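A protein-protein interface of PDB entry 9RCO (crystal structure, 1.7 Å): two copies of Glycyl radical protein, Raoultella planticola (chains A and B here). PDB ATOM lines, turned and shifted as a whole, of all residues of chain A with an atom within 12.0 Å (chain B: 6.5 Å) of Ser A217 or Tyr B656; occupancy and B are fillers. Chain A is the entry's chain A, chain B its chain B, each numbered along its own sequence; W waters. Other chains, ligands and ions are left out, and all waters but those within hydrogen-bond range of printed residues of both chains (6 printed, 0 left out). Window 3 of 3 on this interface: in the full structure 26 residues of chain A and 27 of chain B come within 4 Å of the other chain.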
ATOM      1  N   ALA A 210     -12.191  -3.226   8.328  1.00  0.00           N
ATOM      2  CA  ALA A 210     -13.172  -2.827   7.320  1.00  0.00           C
ATOM      3  C   ALA A 210     -13.365  -1.315   7.317  1.00  0.00           C
ATOM      4  O   ALA A 210     -13.494  -0.701   6.250  1.00  0.00           O
ATOM      5  CB  ALA A 210     -14.507  -3.535   7.560  1.00  0.00           C
ATOM      6  N   LEU A 211     -13.380  -0.706   8.505  1.00  0.00           N
ATOM      7  CA  LEU A 211     -13.423   0.748   8.625  1.00  0.00           C
ATOM      8  C   LEU A 211     -12.202   1.387   7.979  1.00  0.00           C
ATOM      9  O   LEU A 211     -12.317   2.370   7.236  1.00  0.00           O
ATOM     10  CB  LEU A 211     -13.501   1.142  10.099  1.00  0.00           C
ATOM     11  CG  LEU A 211     -14.869   1.083  10.753  1.00  0.00           C
ATOM     12  CD1 LEU A 211     -14.742   1.110  12.264  1.00  0.00           C
ATOM     13  CD2 LEU A 211     -15.692   2.265  10.275  1.00  0.00           C
ATOM     14  N   GLU A 212     -11.015   0.861   8.287  1.00  0.00           N
ATOM     15  CA  GLU A 212      -9.790   1.378   7.689  1.00  0.00           C
ATOM     16  C   GLU A 212      -9.858   1.357   6.166  1.00  0.00           C
ATOM     17  O   GLU A 212      -9.363   2.270   5.499  1.00  0.00           O
ATOM     18  CB  GLU A 212      -8.594   0.571   8.197  1.00  0.00           C
ATOM     19  CG  GLU A 212      -8.071   1.068   9.535  1.00  0.00           C
ATOM     20  CD  GLU A 212      -7.176   0.062  10.234  1.00  0.00           C
ATOM     21  OE1 GLU A 212      -6.624  -0.823   9.544  1.00  0.00           O
ATOM     22  OE2 GLU A 212      -7.012   0.175  11.469  1.00  0.00           O
ATOM     23  N   ASN A 213     -10.477   0.335   5.597  1.00  0.00           N
ATOM     24  CA  ASN A 213     -10.493   0.169   4.151  1.00  0.00           C
ATOM     25  C   ASN A 213     -11.733   0.738   3.479  1.00  0.00           C
ATOM     26  O   ASN A 213     -11.885   0.571   2.267  1.00  0.00           O
ATOM     27  CB  ASN A 213     -10.345  -1.307   3.806  1.00  0.00           C
ATOM     28  CG  ASN A 213      -9.001  -1.842   4.220  1.00  0.00           C
ATOM     29  OD1 ASN A 213      -7.995  -1.130   4.134  1.00  0.00           O
ATOM     30  ND2 ASN A 213      -8.967  -3.081   4.691  1.00  0.00           N
ATOM     31  N   LEU A 214     -12.621   1.390   4.226  1.00  0.00           N
ATOM     32  CA  LEU A 214     -13.839   1.945   3.638  1.00  0.00           C
ATOM     33  C   LEU A 214     -13.528   2.948   2.537  1.00  0.00           C
ATOM     34  O   LEU A 214     -12.725   3.864   2.723  1.00  0.00           O
ATOM     35  CB  LEU A 214     -14.685   2.641   4.699  1.00  0.00           C
ATOM     36  CG  LEU A 214     -15.966   2.026   5.238  1.00  0.00           C
ATOM     37  CD1 LEU A 214     -16.621   3.029   6.200  1.00  0.00           C
ATOM     38  CD2 LEU A 214     -16.893   1.644   4.092  1.00  0.00           C
ATOM     39  N   ASP A 215     -14.192   2.787   1.394  1.00  0.00           N
ATOM     40  CA  ASP A 215     -14.191   3.819   0.357  1.00  0.00           C
ATOM     41  C   ASP A 215     -15.088   4.962   0.805  1.00  0.00           C
ATOM     42  O   ASP A 215     -16.312   4.806   0.878  1.00  0.00           O
ATOM     43  CB  ASP A 215     -14.668   3.222  -0.961  1.00  0.00           C
ATOM     44  CG  ASP A 215     -14.703   4.235  -2.103  1.00  0.00           C
ATOM     45  OD1 ASP A 215     -14.560   5.463  -1.881  1.00  0.00           O
ATOM     46  OD2 ASP A 215     -14.875   3.781  -3.254  1.00  0.00           O
ATOM     47  N   ARG A 216     -14.491   6.117   1.105  1.00  0.00           N
ATOM     48  CA  ARG A 216     -15.246   7.250   1.611  1.00  0.00           C
ATOM     49  C   ARG A 216     -15.442   8.327   0.548  1.00  0.00           C
ATOM     50  O   ARG A 216     -15.737   9.478   0.881  1.00  0.00           O
ATOM     51  CB  ARG A 216     -14.560   7.812   2.856  1.00  0.00           C
ATOM     52  CG  ARG A 216     -14.534   6.802   4.006  1.00  0.00           C
ATOM     53  CD  ARG A 216     -13.604   7.232   5.114  1.00  0.00           C
ATOM     54  NE  ARG A 216     -13.392   6.158   6.082  1.00  0.00           N
ATOM     55  CZ  ARG A 216     -14.030   6.087   7.241  1.00  0.00           C
ATOM     56  NH1 ARG A 216     -14.899   7.028   7.565  1.00  0.00           N
ATOM     57  NH2 ARG A 216     -13.801   5.087   8.075  1.00  0.00           N
ATOM     58  N   SER A 217     -15.326   7.956  -0.727  1.00  0.00           N
ATOM     59  CA  SER A 217     -15.414   8.909  -1.828  1.00  0.00           C
ATOM     60  C   SER A 217     -16.846   9.254  -2.219  1.00  0.00           C
ATOM     61  O   SER A 217     -17.038  10.186  -3.015  1.00  0.00           O
ATOM     62  CB  SER A 217     -14.681   8.372  -3.067  1.00  0.00           C
ATOM     63  OG  SER A 217     -15.288   7.193  -3.552  1.00  0.00           O
ATOM     64  N   THR A 218     -17.844   8.528  -1.709  1.00  0.00           N
ATOM     65  CA  THR A 218     -19.245   8.816  -2.008  1.00  0.00           C
ATOM     66  C   THR A 218     -20.033   8.986  -0.715  1.00  0.00           C
ATOM     67  O   THR A 218     -19.444   9.179   0.352  1.00  0.00           O
ATOM     68  CB  THR A 218     -19.871   7.714  -2.865  1.00  0.00           C
ATOM     69  OG1 THR A 218     -19.965   6.499  -2.104  1.00  0.00           O
ATOM     70  CG2 THR A 218     -19.025   7.456  -4.107  1.00  0.00           C
ATOM     71  N   SER A 219     -21.360   8.968  -0.792  1.00  0.00           N
ATOM     72  CA  SER A 219     -22.142   9.090   0.434  1.00  0.00           C
ATOM     73  C   SER A 219     -22.433   7.745   1.097  1.00  0.00           C
ATOM     74  O   SER A 219     -22.875   7.726   2.255  1.00  0.00           O
ATOM     75  CB  SER A 219     -23.454   9.822   0.156  1.00  0.00           C
ATOM     76  OG  SER A 219     -24.245   9.119  -0.788  1.00  0.00           O
ATOM     77  N   ASP A 220     -22.153   6.631   0.419  1.00  0.00           N
ATOM     78  CA  ASP A 220     -22.492   5.294   0.903  1.00  0.00           C
ATOM     79  C   ASP A 220     -21.761   4.915   2.183  1.00  0.00           C
ATOM     80  O   ASP A 220     -22.212   4.020   2.905  1.00  0.00           O
ATOM     81  CB  ASP A 220     -22.149   4.244  -0.158  1.00  0.00           C
ATOM     82  CG  ASP A 220     -23.178   4.156  -1.267  1.00  0.00           C
ATOM     83  OD1 ASP A 220     -24.265   4.756  -1.143  1.00  0.00           O
ATOM     84  OD2 ASP A 220     -22.886   3.461  -2.267  1.00  0.00           O
ATOM     85  N   TYR A 221     -20.602   5.524   2.450  1.00  0.00           N
ATOM     86  CA  TYR A 221     -19.828   5.103   3.610  1.00  0.00           C
ATOM     87  C   TYR A 221     -20.481   5.497   4.918  1.00  0.00           C
ATOM     88  O   TYR A 221     -20.209   4.867   5.941  1.00  0.00           O
ATOM     89  CB  TYR A 221     -18.413   5.672   3.502  1.00  0.00           C
ATOM     90  CG  TYR A 221     -18.208   7.096   3.994  1.00  0.00           C
ATOM     91  CD1 TYR A 221     -17.961   7.409   5.335  1.00  0.00           C
ATOM     92  CD2 TYR A 221     -18.276   8.148   3.078  1.00  0.00           C
ATOM     93  CE1 TYR A 221     -17.774   8.742   5.732  1.00  0.00           C
ATOM     94  CE2 TYR A 221     -18.090   9.455   3.460  1.00  0.00           C
ATOM     95  CZ  TYR A 221     -17.845   9.757   4.777  1.00  0.00           C
ATOM     96  OH  TYR A 221     -17.671  11.089   5.088  1.00  0.00           O
ATOM     97  N   ILE A 222     -21.356   6.500   4.895  1.00  0.00           N
ATOM     98  CA  ILE A 222     -21.868   7.061   6.139  1.00  0.00           C
ATOM     99  C   ILE A 222     -22.675   6.022   6.905  1.00  0.00           C
ATOM    100  O   ILE A 222     -22.490   5.830   8.117  1.00  0.00           O
ATOM    101  CB  ILE A 222     -22.697   8.316   5.852  1.00  0.00           C
ATOM    102  CG1 ILE A 222     -21.789   9.416   5.293  1.00  0.00           C
ATOM    103  CG2 ILE A 222     -23.451   8.758   7.118  1.00  0.00           C
ATOM    104  CD1 ILE A 222     -22.561  10.585   4.682  1.00  0.00           C
ATOM    105  N   LYS A 223     -23.577   5.325   6.211  1.00  0.00           N
ATOM    106  CA  LYS A 223     -24.375   4.323   6.898  1.00  0.00           C
ATOM    107  C   LYS A 223     -23.565   3.061   7.192  1.00  0.00           C
ATOM    108  O   LYS A 223     -23.787   2.431   8.231  1.00  0.00           O
ATOM    109  CB  LYS A 223     -25.645   3.996   6.102  1.00  0.00           C
ATOM    110  CG  LYS A 223     -26.730   5.101   6.216  1.00  0.00           C
ATOM    111  CD  LYS A 223     -27.989   4.780   5.412  1.00  0.00           C
ATOM    112  CE  LYS A 223     -28.857   3.708   6.092  1.00  0.00           C
ATOM    113  NZ  LYS A 223     -29.543   4.214   7.332  1.00  0.00           N
ATOM    114  N   LYS A 224     -22.604   2.705   6.324  1.00  0.00           N
ATOM    115  CA  LYS A 224     -21.760   1.551   6.613  1.00  0.00           C
ATOM    116  C   LYS A 224     -20.929   1.795   7.858  1.00  0.00           C
ATOM    117  O   LYS A 224     -20.704   0.881   8.663  1.00  0.00           O
ATOM    118  CB  LYS A 224     -20.847   1.244   5.428  1.00  0.00           C
ATOM    119  CG  LYS A 224     -21.593   0.930   4.140  1.00  0.00           C
ATOM    120  CD  LYS A 224     -20.588   0.586   3.036  1.00  0.00           C
ATOM    121  CE  LYS A 224     -21.283   0.246   1.733  1.00  0.00           C
ATOM    122  NZ  LYS A 224     -20.323  -0.119   0.638  1.00  0.00           N
ATOM    123  N   GLU A 225     -20.452   3.025   8.024  1.00  0.00           N
ATOM    124  CA  GLU A 225     -19.672   3.364   9.203  1.00  0.00           C
ATOM    125  C   GLU A 225     -20.519   3.257  10.475  1.00  0.00           C
ATOM    126  O   GLU A 225     -20.038   2.764  11.505  1.00  0.00           O
ATOM    127  CB  GLU A 225     -19.086   4.762   9.011  1.00  0.00           C
ATOM    128  CG  GLU A 225     -18.292   5.298  10.160  1.00  0.00           C
ATOM    129  CD  GLU A 225     -17.177   6.204   9.675  1.00  0.00           C
ATOM    130  OE1 GLU A 225     -17.501   7.235   9.056  1.00  0.00           O
ATOM    131  OE2 GLU A 225     -15.996   5.919   9.957  1.00  0.00           O
ATOM    132  N   ALA B 519      -9.023  19.905   0.626  1.00  0.00           N
ATOM    133  CA  ALA B 519      -9.545  18.555   0.427  1.00  0.00           C
ATOM    134  C   ALA B 519     -10.011  17.949   1.743  1.00  0.00           C
ATOM    135  O   ALA B 519     -11.062  17.302   1.803  1.00  0.00           O
ATOM    136  CB  ALA B 519      -8.479  17.671  -0.223  1.00  0.00           C
ATOM    137  N   VAL B 522     -13.270  19.983   2.824  1.00  0.00           N
ATOM    138  CA  VAL B 522     -14.424  19.793   1.949  1.00  0.00           C
ATOM    139  C   VAL B 522     -14.980  18.375   2.105  1.00  0.00           C
ATOM    140  O   VAL B 522     -16.196  18.159   2.008  1.00  0.00           O
ATOM    141  CB  VAL B 522     -14.068  20.133   0.484  1.00  0.00           C
ATOM    142  CG1 VAL B 522     -15.136  19.625  -0.478  1.00  0.00           C
ATOM    143  CG2 VAL B 522     -13.908  21.671   0.311  1.00  0.00           C
ATOM    144  N   HIS B 523     -14.122  17.383   2.345  1.00  0.00           N
ATOM    145  CA  HIS B 523     -14.656  16.056   2.627  1.00  0.00           C
ATOM    146  C   HIS B 523     -15.563  16.095   3.852  1.00  0.00           C
ATOM    147  O   HIS B 523     -16.647  15.509   3.842  1.00  0.00           O
ATOM    148  CB  HIS B 523     -13.524  15.048   2.808  1.00  0.00           C
ATOM    149  CG  HIS B 523     -13.990  13.629   2.926  1.00  0.00           C
ATOM    150  ND1 HIS B 523     -14.316  13.053   4.135  1.00  0.00           N
ATOM    151  CD2 HIS B 523     -14.183  12.670   1.989  1.00  0.00           C
ATOM    152  CE1 HIS B 523     -14.682  11.796   3.940  1.00  0.00           C
ATOM    153  NE2 HIS B 523     -14.614  11.538   2.645  1.00  0.00           N
ATOM    154  N   VAL B 526     -18.896  17.739   2.975  1.00  0.00           N
ATOM    155  CA  VAL B 526     -19.749  16.816   2.237  1.00  0.00           C
ATOM    156  C   VAL B 526     -20.370  15.790   3.178  1.00  0.00           C
ATOM    157  O   VAL B 526     -21.569  15.480   3.083  1.00  0.00           O
ATOM    158  CB  VAL B 526     -18.919  16.151   1.124  1.00  0.00           C
ATOM    159  CG1 VAL B 526     -19.618  14.919   0.571  1.00  0.00           C
ATOM    160  CG2 VAL B 526     -18.601  17.184   0.043  1.00  0.00           C
ATOM    161  N   ASN B 530     -24.336  15.474   3.696  1.00  0.00           N
ATOM    162  CA  ASN B 530     -24.951  14.194   3.355  1.00  0.00           C
ATOM    163  C   ASN B 530     -25.603  13.556   4.569  1.00  0.00           C
ATOM    164  O   ASN B 530     -26.595  12.826   4.431  1.00  0.00           O
ATOM    165  CB  ASN B 530     -23.921  13.243   2.733  1.00  0.00           C
ATOM    166  CG  ASN B 530     -23.586  13.601   1.277  1.00  0.00           C
ATOM    167  OD1 ASN B 530     -24.365  14.279   0.595  1.00  0.00           O
ATOM    168  ND2 ASN B 530     -22.467  13.083   0.779  1.00  0.00           N
ATOM    169  N   GLU B 652     -12.754  21.231  -5.750  1.00  0.00           N
ATOM    170  CA  GLU B 652     -12.850  20.169  -4.756  1.00  0.00           C
ATOM    171  C   GLU B 652     -14.303  19.793  -4.504  1.00  0.00           C
ATOM    172  O   GLU B 652     -14.635  18.602  -4.400  1.00  0.00           O
ATOM    173  CB  GLU B 652     -12.161  20.589  -3.456  1.00  0.00           C
ATOM    174  CG  GLU B 652     -11.992  19.416  -2.499  1.00  0.00           C
ATOM    175  CD  GLU B 652     -10.893  18.470  -2.936  1.00  0.00           C
ATOM    176  OE1 GLU B 652     -10.090  18.837  -3.824  1.00  0.00           O
ATOM    177  OE2 GLU B 652     -10.863  17.332  -2.433  1.00  0.00           O
ATOM    178  N   VAL B 653     -15.180  20.800  -4.400  1.00  0.00           N
ATOM    179  CA  VAL B 653     -16.590  20.544  -4.119  1.00  0.00           C
ATOM    180  C   VAL B 653     -17.186  19.615  -5.168  1.00  0.00           C
ATOM    181  O   VAL B 653     -17.909  18.665  -4.838  1.00  0.00           O
ATOM    182  CB  VAL B 653     -17.359  21.881  -4.033  1.00  0.00           C
ATOM    183  CG1 VAL B 653     -18.882  21.658  -4.097  1.00  0.00           C
ATOM    184  CG2 VAL B 653     -16.961  22.629  -2.761  1.00  0.00           C
ATOM    185  N   GLU B 654     -16.869  19.847  -6.451  1.00  0.00           N
ATOM    186  CA  GLU B 654     -17.580  19.123  -7.504  1.00  0.00           C
ATOM    187  C   GLU B 654     -17.182  17.657  -7.597  1.00  0.00           C
ATOM    188  O   GLU B 654     -17.775  16.933  -8.396  1.00  0.00           O
ATOM    189  CB  GLU B 654     -17.381  19.778  -8.884  1.00  0.00           C
ATOM    190  CG  GLU B 654     -15.922  20.030  -9.293  1.00  0.00           C
ATOM    191  CD  GLU B 654     -15.777  20.441 -10.765  1.00  0.00           C
ATOM    192  OE1 GLU B 654     -16.726  21.040 -11.318  1.00  0.00           O
ATOM    193  OE2 GLU B 654     -14.681  20.255 -11.340  1.00  0.00           O
ATOM    194  N   LYS B 655     -16.202  17.202  -6.812  1.00  0.00           N
ATOM    195  CA  LYS B 655     -15.793  15.799  -6.836  1.00  0.00           C
ATOM    196  C   LYS B 655     -16.753  14.882  -6.090  1.00  0.00           C
ATOM    197  O   LYS B 655     -16.566  13.660  -6.113  1.00  0.00           O
ATOM    198  CB  LYS B 655     -14.397  15.659  -6.218  1.00  0.00           C
ATOM    199  CG  LYS B 655     -13.289  16.365  -7.007  1.00  0.00           C
ATOM    200  CD  LYS B 655     -11.991  16.383  -6.214  1.00  0.00           C
ATOM    201  CE  LYS B 655     -10.868  17.036  -6.995  1.00  0.00           C
ATOM    202  NZ  LYS B 655      -9.606  17.119  -6.201  1.00  0.00           N
ATOM    203  N   TYR B 656     -17.756  15.431  -5.420  1.00  0.00           N
ATOM    204  CA  TYR B 656     -18.532  14.673  -4.453  1.00  0.00           C
ATOM    205  C   TYR B 656     -19.985  14.558  -4.882  1.00  0.00           C
ATOM    206  O   TYR B 656     -20.489  15.357  -5.681  1.00  0.00           O
ATOM    207  CB  TYR B 656     -18.435  15.315  -3.067  1.00  0.00           C
ATOM    208  CG  TYR B 656     -17.055  15.126  -2.495  1.00  0.00           C
ATOM    209  CD1 TYR B 656     -16.683  13.896  -1.957  1.00  0.00           C
ATOM    210  CD2 TYR B 656     -16.109  16.148  -2.532  1.00  0.00           C
ATOM    211  CE1 TYR B 656     -15.418  13.693  -1.439  1.00  0.00           C
ATOM    212  CE2 TYR B 656     -14.833  15.952  -2.015  1.00  0.00           C
ATOM    213  CZ  TYR B 656     -14.500  14.725  -1.467  1.00  0.00           C
ATOM    214  OH  TYR B 656     -13.243  14.497  -0.949  1.00  0.00           O
ATOM    215  N   THR B 657     -20.647  13.533  -4.332  1.00  0.00           N
ATOM    216  CA  THR B 657     -22.038  13.241  -4.637  1.00  0.00           C
ATOM    217  C   THR B 657     -22.862  13.104  -3.360  1.00  0.00           C
ATOM    218  O   THR B 657     -22.327  12.923  -2.259  1.00  0.00           O
ATOM    219  CB  THR B 657     -22.179  11.961  -5.479  1.00  0.00           C
ATOM    220  OG1 THR B 657     -21.565  10.872  -4.799  1.00  0.00           O
ATOM    221  CG2 THR B 657     -21.521  12.133  -6.847  1.00  0.00           C
ATOM    222  N   ASN B 658     -24.182  13.169  -3.520  1.00  0.00           N
ATOM    223  CA  ASN B 658     -25.116  13.100  -2.408  1.00  0.00           C
ATOM    224  C   ASN B 658     -25.932  11.809  -2.490  1.00  0.00           C
ATOM    225  O   ASN B 658     -25.832  11.063  -3.473  1.00  0.00           O
ATOM    226  CB  ASN B 658     -26.003  14.365  -2.363  1.00  0.00           C
ATOM    227  CG  ASN B 658     -26.909  14.544  -3.573  1.00  0.00           C
ATOM    228  OD1 ASN B 658     -27.498  13.601  -4.091  1.00  0.00           O
ATOM    229  ND2 ASN B 658     -26.995  15.801  -4.048  1.00  0.00           N
ATOM    230  N   GLY B 662     -27.035  12.678  -6.770  1.00  0.00           N
ATOM    231  CA  GLY B 662     -26.709  13.947  -7.373  1.00  0.00           C
ATOM    232  C   GLY B 662     -25.324  14.444  -6.991  1.00  0.00           C
ATOM    233  O   GLY B 662     -24.598  13.841  -6.211  1.00  0.00           O
ATOM    234  N   ARG B 663     -24.993  15.605  -7.545  1.00  0.00           N
ATOM    235  CA  ARG B 663     -23.637  16.133  -7.592  1.00  0.00           C
ATOM    236  C   ARG B 663     -23.533  17.374  -6.715  1.00  0.00           C
ATOM    237  O   ARG B 663     -24.406  18.250  -6.757  1.00  0.00           O
ATOM    238  CB  ARG B 663     -23.288  16.471  -9.048  1.00  0.00           C
ATOM    239  CG  ARG B 663     -21.964  17.190  -9.296  1.00  0.00           C
ATOM    240  CD  ARG B 663     -20.778  16.310  -8.983  1.00  0.00           C
ATOM    241  NE  ARG B 663     -20.838  15.023  -9.673  1.00  0.00           N
ATOM    242  CZ  ARG B 663     -19.936  14.056  -9.522  1.00  0.00           C
ATOM    243  NH1 ARG B 663     -18.897  14.243  -8.719  1.00  0.00           N
ATOM    244  NH2 ARG B 663     -20.059  12.910 -10.184  1.00  0.00           N
ATOM    245  N   PHE B 664     -22.467  17.462  -5.924  1.00  0.00           N
ATOM    246  CA  PHE B 664     -22.160  18.731  -5.271  1.00  0.00           C
ATOM    247  C   PHE B 664     -21.669  19.752  -6.294  1.00  0.00           C
ATOM    248  O   PHE B 664     -20.915  19.419  -7.216  1.00  0.00           O
ATOM    249  CB  PHE B 664     -21.097  18.571  -4.184  1.00  0.00           C
ATOM    250  CG  PHE B 664     -21.605  17.994  -2.896  1.00  0.00           C
ATOM    251  CD1 PHE B 664     -22.103  16.701  -2.822  1.00  0.00           C
ATOM    252  CD2 PHE B 664     -21.652  18.801  -1.768  1.00  0.00           C
ATOM    253  CE1 PHE B 664     -22.576  16.205  -1.596  1.00  0.00           C
ATOM    254  CE2 PHE B 664     -22.122  18.326  -0.566  1.00  0.00           C
ATOM    255  CZ  PHE B 664     -22.598  17.036  -0.480  1.00  0.00           C
ATOM    256  N   GLN B 665     -22.099  21.005  -6.123  1.00  0.00           N
ATOM    257  CA  GLN B 665     -21.654  22.113  -6.963  1.00  0.00           C
ATOM    258  C   GLN B 665     -21.557  23.377  -6.112  1.00  0.00           C
ATOM    259  O   GLN B 665     -22.497  23.721  -5.381  1.00  0.00           O
ATOM    260  CB  GLN B 665     -22.608  22.307  -8.156  1.00  0.00           C
ATOM    261  CG  GLN B 665     -24.064  22.296  -7.714  1.00  0.00           C
ATOM    262  CD  GLN B 665     -25.057  22.842  -8.733  1.00  0.00           C
ATOM    263  OE1 GLN B 665     -24.722  23.113  -9.894  1.00  0.00           O
ATOM    264  NE2 GLN B 665     -26.265  23.110  -8.260  1.00  0.00           N
HETATM  265  O   HOH W   1     -20.329  11.807   1.975  1.00  0.00           O
HETATM  266  O   HOH W   2     -18.886  11.068  -5.012  1.00  0.00           O
HETATM  267  O   HOH W   3     -17.719  12.875   2.805  1.00  0.00           O
HETATM  268  O   HOH W   4     -15.400  11.634  -4.612  1.00  0.00           O
HETATM  269  O   HOH W   5     -22.990   9.082  -3.264  1.00  0.00           O
HETATM  270  O   HOH W   6     -19.645  12.072  -1.828  1.00  0.00           O
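O of Leu A211 sits at hydrogen-bond distance from NH2 of Arg A216, 3.2 Å away.
The side-chain hydroxyl of Ser A217 sits at hydrogen-bond distance from the side-chain carboxylate of Asp A215 (2.5 Å).
The guanidinium group of Arg A216 lies within salt-bridge range of the side-chain carboxylate of Glu A225, at 2.9 Å.
The backbone carbonyl oxygen (O) of Val B526 sits close to the side-chain amide nitrogen (ND2) of Asn B530, 3.4 Å away.
O of Thr B657 sits at hydrogen-bond distance from ND2 of Asn B530.
The backbone carbonyl oxygen of Tyr B656 is in hydrogen-bond range of the backbone NH of Phe B664 (2.9 Å).
The backbone carbonyl oxygen of Arg A216 lies within hydrogen-bond range of a ring nitrogen (NE2) of His B523 (2.9 Å).
Among the printed residues, merely in contact across the chains: Tyr A221 with His B523, Ser A219 with Asn B530, Ile A222 with Asn B530, Ser A219 with Asn B658 and Ser A217 with Tyr B656.
Of the printed residues of chain B, Arg A216 touches His B523.
Ser A217 touches one residue of chain B.
Of the printed residues of chain B, Ser A219 touches Asn B530 (3.5 Å) and Asn B658 (3.6 Å).
Of the printed residues of chain B, Tyr A221 touches His B523.
Ala B519 touches none of the printed residues of chain A.
Val B522 touches none of the printed residues of chain A.
His B523 touches just these residues of chain A: Arg A216 and Tyr A221.
Of the printed residues of chain A, Asn B530 touches Ser A219 (3.5 Å) and Ile A222 (3.6 Å).
No residue of chain A comes within 4 Å of Glu B652.
No residue of chain A comes within 4 Å of Val B653.
No residue of chain A comes within 4 Å of Lys B655.
Of chain A, only Ser A217 (3.9 Å) comes within 4 Å of Tyr B656.
Asn B658 touches just one residue of chain A: Ser A219.
Gly B662 touches none of the printed residues of chain A.
No residue of chain A comes within 4 Å of Arg B663.
No residue of chain A comes within 4 Å of Phe B664.
The nearest residue of chain B that does not touch Ser A217 is Lys B655 (4.7 Å).
The nearest printed residue of chain B that does not touch Tyr A221 is Val B526 (5.7 Å).
Of the 16 printed residues of chain A, 5 touch a printed residue of chain B.
Hydrophobic or aromatic side chains of chain A within 4 Å of the printed part of chain B: Tyr A221 and Ile A222.
Printed residues of chain B that touch a printed residue of chain A: His B523, Asn B530, Tyr B656 and Asn B658.
Among the printed residues, no Asp or Glu carboxylate lies within 4 Å of a Lys or Arg side-chain nitrogen of the other chain.
No position is printed for both chains.
Water W2 bridges the side-chain hydroxyl (OG1) of Thr B657 (2.7 Å) and the backbone carbonyl oxygen (O) of Ser A217 (2.9 Å).
Water W4 lies within hydrogen-bond range of O of Ser A217 (2.7 Å) and O of Lys B655 (2.8 Å).
Water W5 lies within hydrogen-bond range of OG1 of Thr B657 (2.8 Å), OG of Ser A219 (2.8 Å) and O of Asn B658 (3.5 Å).
Water W1 lies within hydrogen-bond range of the side-chain amide nitrogen of Asn B530 (2.8 Å) and the backbone carbonyl oxygen of Thr A218 (3.2 Å).
Water W6 lies within hydrogen-bond range of the backbone carbonyl oxygen (O) of Thr B657 (2.8 Å) and the backbone carbonyl oxygen (O) of Ser A217 (3.4 Å).
Water W3 bridges the side-chain hydroxyl (OH) of Tyr A221 (2.9 Å) and the backbone carbonyl oxygen (O) of His B523 (3.0 Å).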
